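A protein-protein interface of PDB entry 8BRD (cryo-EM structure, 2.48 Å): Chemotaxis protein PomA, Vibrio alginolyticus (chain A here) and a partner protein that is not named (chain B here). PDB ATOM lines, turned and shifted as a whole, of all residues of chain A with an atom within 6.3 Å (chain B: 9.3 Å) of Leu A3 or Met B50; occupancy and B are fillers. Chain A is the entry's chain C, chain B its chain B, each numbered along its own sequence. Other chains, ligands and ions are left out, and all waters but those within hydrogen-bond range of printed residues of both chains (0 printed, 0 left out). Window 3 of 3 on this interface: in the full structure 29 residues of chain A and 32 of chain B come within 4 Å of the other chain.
The side-chain carboxylate (OE2) of Glu A250 sits at hydrogen-bond distance from the side-chain hydroxyl (OG1) of Thr B49 (3.1 Å).
OG1 of Thr B49 is in hydrogen-bond range of N of Gln B52, 3.0 Å away.
Among the printed residues, pairs that only touch across the chains: Gly A8 with Phe B42, Ala A4 with Phe B42, Leu A3 with Met B50, Leu A7 with Phe B42, Glu A250 with Gly B51, Ala A4 with Leu B45, Leu A7 with Leu B45, Glu A250 with Gln B52, Leu A7 with Ile B41 and Ala A4 with Met B46.
Met A1 touches none of the printed residues of chain B.
No residue of chain B comes within 4 Å of Asp A2.
Ala A4 touches just these residues of chain B: Phe B42, Leu B45 and Met B46.
Leu A6 touches none of the printed residues of chain B.
Of the printed residues of chain B, Leu A7 touches Ile B41, Phe B42 and Leu B45.
Printed residues of chain B within 4 Å of Glu A250: Thr B49 (3.1 Å), Gly B51 (3.7 Å) and Gln B52 (3.8 Å).
Printed residues of chain A within 4 Å of Phe B42: Ala A4, Leu A7 and Gly A8.
Printed residues of chain A within 4 Å of Leu B45: Ala A4 (3.8 Å) and Leu A7 (3.8 Å).
Of chain A, only Leu A3 (3.5 Å) comes within 4 Å of Met B50.
The nearest printed residue of chain A that does not touch Thr B49 is Ala A4 (7.6 Å).
Of the 9 printed residues of chain A, 5 touch a printed residue of chain B.
Hydrophobic or aromatic side chains of chain A that line the printed part of chain B: Leu A3, Ala A4 and Leu A7.
Among the printed residues, no Asp or Glu carboxylate lies within 4 Å of a Lys or Arg side-chain nitrogen of the other chain.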
ATOM      1  N   MET A   1      10.435 -33.451  -9.169  1.00  0.00           N
ATOM      2  CA  MET A   1       9.573 -32.320  -8.847  1.00  0.00           C
ATOM      3  C   MET A   1      10.370 -31.172  -8.237  1.00  0.00           C
ATOM      4  O   MET A   1      10.523 -31.091  -7.018  1.00  0.00           O
ATOM      5  CB  MET A   1       8.461 -32.751  -7.888  1.00  0.00           C
ATOM      6  CG  MET A   1       7.093 -32.890  -8.537  1.00  0.00           C
ATOM      7  SD  MET A   1       6.222 -31.317  -8.686  1.00  0.00           S
ATOM      8  CE  MET A   1       5.730 -31.032  -6.991  1.00  0.00           C
ATOM      9  N   ASP A   2      10.874 -30.282  -9.089  1.00  0.00           N
ATOM     10  CA  ASP A   2      11.624 -29.128  -8.622  1.00  0.00           C
ATOM     11  C   ASP A   2      10.666 -28.070  -8.076  1.00  0.00           C
ATOM     12  O   ASP A   2       9.442 -28.220  -8.117  1.00  0.00           O
ATOM     13  CB  ASP A   2      12.492 -28.561  -9.743  1.00  0.00           C
ATOM     14  CG  ASP A   2      11.719 -28.343 -11.027  1.00  0.00           C
ATOM     15  OD1 ASP A   2      10.864 -29.191 -11.360  1.00  0.00           O
ATOM     16  OD2 ASP A   2      11.967 -27.326 -11.704  1.00  0.00           O
ATOM     17  N   LEU A   3      11.233 -26.987  -7.543  1.00  0.00           N
ATOM     18  CA  LEU A   3      10.404 -25.933  -6.970  1.00  0.00           C
ATOM     19  C   LEU A   3       9.608 -25.214  -8.051  1.00  0.00           C
ATOM     20  O   LEU A   3       8.461 -24.811  -7.828  1.00  0.00           O
ATOM     21  CB  LEU A   3      11.270 -24.943  -6.189  1.00  0.00           C
ATOM     22  CG  LEU A   3      10.553 -23.664  -5.752  1.00  0.00           C
ATOM     23  CD1 LEU A   3      10.034 -23.813  -4.332  1.00  0.00           C
ATOM     24  CD2 LEU A   3      11.461 -22.457  -5.862  1.00  0.00           C
ATOM     25  N   ALA A   4      10.200 -25.052  -9.236  1.00  0.00           N
ATOM     26  CA  ALA A   4       9.516 -24.365 -10.327  1.00  0.00           C
ATOM     27  C   ALA A   4       8.221 -25.076 -10.698  1.00  0.00           C
ATOM     28  O   ALA A   4       7.176 -24.443 -10.868  1.00  0.00           O
ATOM     29  CB  ALA A   4      10.443 -24.257 -11.539  1.00  0.00           C
ATOM     30  N   THR A   5       8.275 -26.404 -10.821  1.00  0.00           N
ATOM     31  CA  THR A   5       7.062 -27.177 -11.068  1.00  0.00           C
ATOM     32  C   THR A   5       6.095 -27.078  -9.894  1.00  0.00           C
ATOM     33  O   THR A   5       4.882 -26.928 -10.085  1.00  0.00           O
ATOM     34  CB  THR A   5       7.423 -28.638 -11.337  1.00  0.00           C
ATOM     35  OG1 THR A   5       8.452 -28.702 -12.331  1.00  0.00           O
ATOM     36  CG2 THR A   5       6.209 -29.409 -11.820  1.00  0.00           C
ATOM     37  N   LEU A   6       6.619 -27.168  -8.673  1.00  0.00           N
ATOM     38  CA  LEU A   6       5.789 -27.057  -7.479  1.00  0.00           C
ATOM     39  C   LEU A   6       5.143 -25.679  -7.394  1.00  0.00           C
ATOM     40  O   LEU A   6       3.939 -25.555  -7.128  1.00  0.00           O
ATOM     41  CB  LEU A   6       6.652 -27.341  -6.248  1.00  0.00           C
ATOM     42  CG  LEU A   6       6.328 -26.789  -4.863  1.00  0.00           C
ATOM     43  CD1 LEU A   6       5.272 -27.643  -4.194  1.00  0.00           C
ATOM     44  CD2 LEU A   6       7.584 -26.719  -4.008  1.00  0.00           C
ATOM     45  N   LEU A   7       5.929 -24.632  -7.639  1.00  0.00           N
ATOM     46  CA  LEU A   7       5.421 -23.269  -7.647  1.00  0.00           C
ATOM     47  C   LEU A   7       4.350 -23.121  -8.716  1.00  0.00           C
ATOM     48  O   LEU A   7       3.337 -22.464  -8.488  1.00  0.00           O
ATOM     49  CB  LEU A   7       6.558 -22.271  -7.879  1.00  0.00           C
ATOM     50  CG  LEU A   7       6.228 -20.935  -8.547  1.00  0.00           C
ATOM     51  CD1 LEU A   7       5.521 -19.991  -7.587  1.00  0.00           C
ATOM     52  CD2 LEU A   7       7.496 -20.303  -9.082  1.00  0.00           C
ATOM     53  N   GLY A   8       4.561 -23.742  -9.877  1.00  0.00           N
ATOM     54  CA  GLY A   8       3.571 -23.667 -10.938  1.00  0.00           C
ATOM     55  C   GLY A   8       2.267 -24.348 -10.579  1.00  0.00           C
ATOM     56  O   GLY A   8       1.187 -23.845 -10.887  1.00  0.00           O
ATOM     57  N   GLU A 250      25.982 -18.803 -12.215  1.00  0.00           N
ATOM     58  CA  GLU A 250      26.049 -19.585 -10.989  1.00  0.00           C
ATOM     59  C   GLU A 250      27.408 -19.508 -10.306  1.00  0.00           C
ATOM     60  O   GLU A 250      27.548 -20.011  -9.186  1.00  0.00           O
ATOM     61  CB  GLU A 250      25.711 -21.048 -11.281  1.00  0.00           C
ATOM     62  CG  GLU A 250      24.272 -21.286 -11.709  1.00  0.00           C
ATOM     63  CD  GLU A 250      24.145 -22.401 -12.728  1.00  0.00           C
ATOM     64  OE1 GLU A 250      25.155 -22.712 -13.393  1.00  0.00           O
ATOM     65  OE2 GLU A 250      23.042 -22.966 -12.864  1.00  0.00           O
ATOM     66  N   ILE B  41       7.406 -15.158 -12.237  1.00  0.00           N
ATOM     67  CA  ILE B  41       8.430 -15.919 -11.532  1.00  0.00           C
ATOM     68  C   ILE B  41       8.394 -17.377 -11.959  1.00  0.00           C
ATOM     69  O   ILE B  41       9.437 -17.993 -12.187  1.00  0.00           O
ATOM     70  CB  ILE B  41       8.257 -15.766 -10.009  1.00  0.00           C
ATOM     71  CG1 ILE B  41       8.669 -14.362  -9.566  1.00  0.00           C
ATOM     72  CG2 ILE B  41       9.066 -16.813  -9.269  1.00  0.00           C
ATOM     73  CD1 ILE B  41       8.632 -14.154  -8.075  1.00  0.00           C
ATOM     74  N   PHE B  42       7.197 -17.949 -12.081  1.00  0.00           N
ATOM     75  CA  PHE B  42       7.077 -19.329 -12.532  1.00  0.00           C
ATOM     76  C   PHE B  42       7.659 -19.503 -13.929  1.00  0.00           C
ATOM     77  O   PHE B  42       8.462 -20.409 -14.167  1.00  0.00           O
ATOM     78  CB  PHE B  42       5.613 -19.765 -12.498  1.00  0.00           C
ATOM     79  CG  PHE B  42       5.315 -20.943 -13.372  1.00  0.00           C
ATOM     80  CD1 PHE B  42       5.749 -22.208 -13.027  1.00  0.00           C
ATOM     81  CD2 PHE B  42       4.613 -20.787 -14.549  1.00  0.00           C
ATOM     82  CE1 PHE B  42       5.472 -23.290 -13.831  1.00  0.00           C
ATOM     83  CE2 PHE B  42       4.337 -21.864 -15.357  1.00  0.00           C
ATOM     84  CZ  PHE B  42       4.769 -23.117 -15.000  1.00  0.00           C
ATOM     85  N   VAL B  44       9.824 -17.650 -15.559  1.00  0.00           N
ATOM     86  CA  VAL B  44      11.261 -17.407 -15.593  1.00  0.00           C
ATOM     87  C   VAL B  44      12.021 -18.552 -14.935  1.00  0.00           C
ATOM     88  O   VAL B  44      13.097 -18.944 -15.397  1.00  0.00           O
ATOM     89  CB  VAL B  44      11.576 -16.043 -14.947  1.00  0.00           C
ATOM     90  CG1 VAL B  44      13.070 -15.854 -14.772  1.00  0.00           C
ATOM     91  CG2 VAL B  44      11.003 -14.926 -15.795  1.00  0.00           C
ATOM     92  N   LEU B  45      11.476 -19.119 -13.856  1.00  0.00           N
ATOM     93  CA  LEU B  45      12.109 -20.260 -13.209  1.00  0.00           C
ATOM     94  C   LEU B  45      11.997 -21.530 -14.035  1.00  0.00           C
ATOM     95  O   LEU B  45      12.793 -22.452 -13.840  1.00  0.00           O
ATOM     96  CB  LEU B  45      11.501 -20.490 -11.830  1.00  0.00           C
ATOM     97  CG  LEU B  45      11.926 -19.514 -10.737  1.00  0.00           C
ATOM     98  CD1 LEU B  45      11.252 -19.873  -9.430  1.00  0.00           C
ATOM     99  CD2 LEU B  45      13.434 -19.514 -10.594  1.00  0.00           C
ATOM    100  N   MET B  46      11.013 -21.615 -14.930  1.00  0.00           N
ATOM    101  CA  MET B  46      11.016 -22.705 -15.899  1.00  0.00           C
ATOM    102  C   MET B  46      12.060 -22.468 -16.981  1.00  0.00           C
ATOM    103  O   MET B  46      12.658 -23.419 -17.488  1.00  0.00           O
ATOM    104  CB  MET B  46       9.625 -22.883 -16.507  1.00  0.00           C
ATOM    105  CG  MET B  46       8.531 -23.080 -15.473  1.00  0.00           C
ATOM    106  SD  MET B  46       8.346 -24.738 -14.794  1.00  0.00           S
ATOM    107  CE  MET B  46       8.694 -25.726 -16.232  1.00  0.00           C
ATOM    108  N   LYS B  47      12.298 -21.202 -17.343  1.00  0.00           N
ATOM    109  CA  LYS B  47      13.335 -20.901 -18.330  1.00  0.00           C
ATOM    110  C   LYS B  47      14.739 -21.002 -17.744  1.00  0.00           C
ATOM    111  O   LYS B  47      15.663 -21.453 -18.424  1.00  0.00           O
ATOM    112  CB  LYS B  47      13.134 -19.504 -18.918  1.00  0.00           C
ATOM    113  CG  LYS B  47      11.821 -19.284 -19.623  1.00  0.00           C
ATOM    114  CD  LYS B  47      11.863 -18.015 -20.456  1.00  0.00           C
ATOM    115  CE  LYS B  47      10.481 -17.621 -20.940  1.00  0.00           C
ATOM    116  NZ  LYS B  47       9.881 -18.648 -21.835  1.00  0.00           N
ATOM    117  N   PHE B  48      14.925 -20.566 -16.503  1.00  0.00           N
ATOM    118  CA  PHE B  48      16.244 -20.451 -15.903  1.00  0.00           C
ATOM    119  C   PHE B  48      16.288 -21.226 -14.598  1.00  0.00           C
ATOM    120  O   PHE B  48      15.269 -21.414 -13.933  1.00  0.00           O
ATOM    121  CB  PHE B  48      16.616 -18.983 -15.641  1.00  0.00           C
ATOM    122  CG  PHE B  48      16.653 -18.140 -16.878  1.00  0.00           C
ATOM    123  CD1 PHE B  48      17.791 -18.084 -17.658  1.00  0.00           C
ATOM    124  CD2 PHE B  48      15.546 -17.409 -17.268  1.00  0.00           C
ATOM    125  CE1 PHE B  48      17.825 -17.317 -18.797  1.00  0.00           C
ATOM    126  CE2 PHE B  48      15.576 -16.644 -18.407  1.00  0.00           C
ATOM    127  CZ  PHE B  48      16.717 -16.597 -19.174  1.00  0.00           C
ATOM    128  N   THR B  49      17.484 -21.676 -14.234  1.00  0.00           N
ATOM    129  CA  THR B  49      17.659 -22.363 -12.967  1.00  0.00           C
ATOM    130  C   THR B  49      17.563 -21.360 -11.820  1.00  0.00           C
ATOM    131  O   THR B  49      17.548 -20.143 -12.018  1.00  0.00           O
ATOM    132  CB  THR B  49      18.998 -23.094 -12.936  1.00  0.00           C
ATOM    133  OG1 THR B  49      20.061 -22.140 -12.884  1.00  0.00           O
ATOM    134  CG2 THR B  49      19.160 -23.945 -14.180  1.00  0.00           C
ATOM    135  N   MET B  50      17.478 -21.883 -10.599  1.00  0.00           N
ATOM    136  CA  MET B  50      17.481 -21.011  -9.432  1.00  0.00           C
ATOM    137  C   MET B  50      18.820 -20.304  -9.275  1.00  0.00           C
ATOM    138  O   MET B  50      18.858 -19.123  -8.906  1.00  0.00           O
ATOM    139  CB  MET B  50      17.150 -21.817  -8.180  1.00  0.00           C
ATOM    140  CG  MET B  50      16.932 -20.973  -6.945  1.00  0.00           C
ATOM    141  SD  MET B  50      15.339 -20.141  -6.965  1.00  0.00           S
ATOM    142  CE  MET B  50      14.322 -21.427  -7.676  1.00  0.00           C
ATOM    143  N   GLY B  51      19.920 -21.006  -9.549  1.00  0.00           N
ATOM    144  CA  GLY B  51      21.227 -20.378  -9.485  1.00  0.00           C
ATOM    145  C   GLY B  51      21.391 -19.264 -10.499  1.00  0.00           C
ATOM    146  O   GLY B  51      21.950 -18.210 -10.189  1.00  0.00           O
ATOM    147  N   GLN B  52      20.903 -19.477 -11.723  1.00  0.00           N
ATOM    148  CA  GLN B  52      20.942 -18.419 -12.728  1.00  0.00           C
ATOM    149  C   GLN B  52      20.137 -17.206 -12.288  1.00  0.00           C
ATOM    150  O   GLN B  52      20.595 -16.069 -12.421  1.00  0.00           O
ATOM    151  CB  GLN B  52      20.416 -18.938 -14.064  1.00  0.00           C
ATOM    152  CG  GLN B  52      21.387 -19.796 -14.834  1.00  0.00           C
ATOM    153  CD  GLN B  52      20.819 -20.255 -16.155  1.00  0.00           C
ATOM    154  OE1 GLN B  52      19.977 -21.149 -16.207  1.00  0.00           O
ATOM    155  NE2 GLN B  52      21.275 -19.640 -17.238  1.00  0.00           N
ATOM    156  N   PHE B  53      18.933 -17.429 -11.760  1.00  0.00           N
ATOM    157  CA  PHE B  53      18.091 -16.318 -11.331  1.00  0.00           C
ATOM    158  C   PHE B  53      18.738 -15.539 -10.189  1.00  0.00           C
ATOM    159  O   PHE B  53      18.739 -14.300 -10.193  1.00  0.00           O
ATOM    160  CB  PHE B  53      16.715 -16.844 -10.926  1.00  0.00           C
ATOM    161  CG  PHE B  53      15.892 -15.864 -10.147  1.00  0.00           C
ATOM    162  CD1 PHE B  53      15.212 -14.847 -10.790  1.00  0.00           C
ATOM    163  CD2 PHE B  53      15.785 -15.969  -8.772  1.00  0.00           C
ATOM    164  CE1 PHE B  53      14.452 -13.946 -10.077  1.00  0.00           C
ATOM    165  CE2 PHE B  53      15.028 -15.071  -8.054  1.00  0.00           C
ATOM    166  CZ  PHE B  53      14.359 -14.058  -8.708  1.00  0.00           C
ATOM    167  N   PHE B  54      19.311 -16.243  -9.213  1.00  0.00           N
ATOM    168  CA  PHE B  54      19.939 -15.551  -8.093  1.00  0.00           C
ATOM    169  C   PHE B  54      21.208 -14.829  -8.525  1.00  0.00           C
ATOM    170  O   PHE B  54      21.488 -13.724  -8.050  1.00  0.00           O
ATOM    171  CB  PHE B  54      20.220 -16.536  -6.963  1.00  0.00           C
ATOM    172  CG  PHE B  54      19.018 -16.832  -6.119  1.00  0.00           C
ATOM    173  CD1 PHE B  54      18.112 -15.832  -5.820  1.00  0.00           C
ATOM    174  CD2 PHE B  54      18.786 -18.103  -5.636  1.00  0.00           C
ATOM    175  CE1 PHE B  54      16.999 -16.093  -5.052  1.00  0.00           C
ATOM    176  CE2 PHE B  54      17.675 -18.370  -4.862  1.00  0.00           C
ATOM    177  CZ  PHE B  54      16.780 -17.363  -4.573  1.00  0.00           C
ATOM    178  N   GLY B  55      21.985 -15.425  -9.430  1.00  0.00           N
ATOM    179  CA  GLY B  55      23.142 -14.727  -9.959  1.00  0.00           C
ATOM    180  C   GLY B  55      22.761 -13.481 -10.733  1.00  0.00           C
ATOM    181  O   GLY B  55      23.445 -12.458 -10.657  1.00  0.00           O
ATOM    182  N   ALA B  56      21.667 -13.552 -11.494  1.00  0.00           N
ATOM    183  CA  ALA B  56      21.174 -12.375 -12.200  1.00  0.00           C
ATOM    184  C   ALA B  56      20.758 -11.290 -11.223  1.00  0.00           C
ATOM    185  O   ALA B  56      21.035 -10.107 -11.443  1.00  0.00           O
ATOM    186  CB  ALA B  56      20.006 -12.755 -13.108  1.00  0.00           C
ATOM    187  N   THR B  57      20.090 -11.672 -10.135  1.00  0.00           N
ATOM    188  CA  THR B  57      19.729 -10.694  -9.114  1.00  0.00           C
ATOM    189  C   THR B  57      20.968 -10.050  -8.499  1.00  0.00           C
ATOM    190  O   THR B  57      21.013  -8.827  -8.314  1.00  0.00           O
ATOM    191  CB  THR B  57      18.873 -11.360  -8.037  1.00  0.00           C
ATOM    192  OG1 THR B  57      17.512 -11.421  -8.482  1.00  0.00           O
ATOM    193  CG2 THR B  57      18.939 -10.585  -6.736  1.00  0.00           C
ATOM    194  N   LYS B  58      21.988 -10.854  -8.190  1.00  0.00           N
ATOM    195  CA  LYS B  58      23.209 -10.306  -7.604  1.00  0.00           C
ATOM    196  C   LYS B  58      23.898  -9.349  -8.568  1.00  0.00           C
ATOM    197  O   LYS B  58      24.352  -8.271  -8.171  1.00  0.00           O
ATOM    198  CB  LYS B  58      24.166 -11.429  -7.197  1.00  0.00           C
ATOM    199  CG  LYS B  58      23.589 -12.457  -6.235  1.00  0.00           C
ATOM    200  CD  LYS B  58      22.718 -11.817  -5.172  1.00  0.00           C
ATOM    201  CE  LYS B  58      22.042 -12.870  -4.309  1.00  0.00           C
ATOM    202  NZ  LYS B  58      21.039 -12.266  -3.390  1.00  0.00           N
ATOM    203  N   VAL B 140      17.776 -13.066 -18.318  1.00  0.00           N
ATOM    204  CA  VAL B 140      16.816 -13.331 -17.248  1.00  0.00           C
ATOM    205  C   VAL B 140      15.836 -12.170 -17.110  1.00  0.00           C
ATOM    206  O   VAL B 140      14.613 -12.363 -17.036  1.00  0.00           O
ATOM    207  CB  VAL B 140      17.553 -13.600 -15.924  1.00  0.00           C
ATOM    208  CG1 VAL B 140      16.583 -13.589 -14.762  1.00  0.00           C
ATOM    209  CG2 VAL B 140      18.290 -14.917 -15.986  1.00  0.00           C
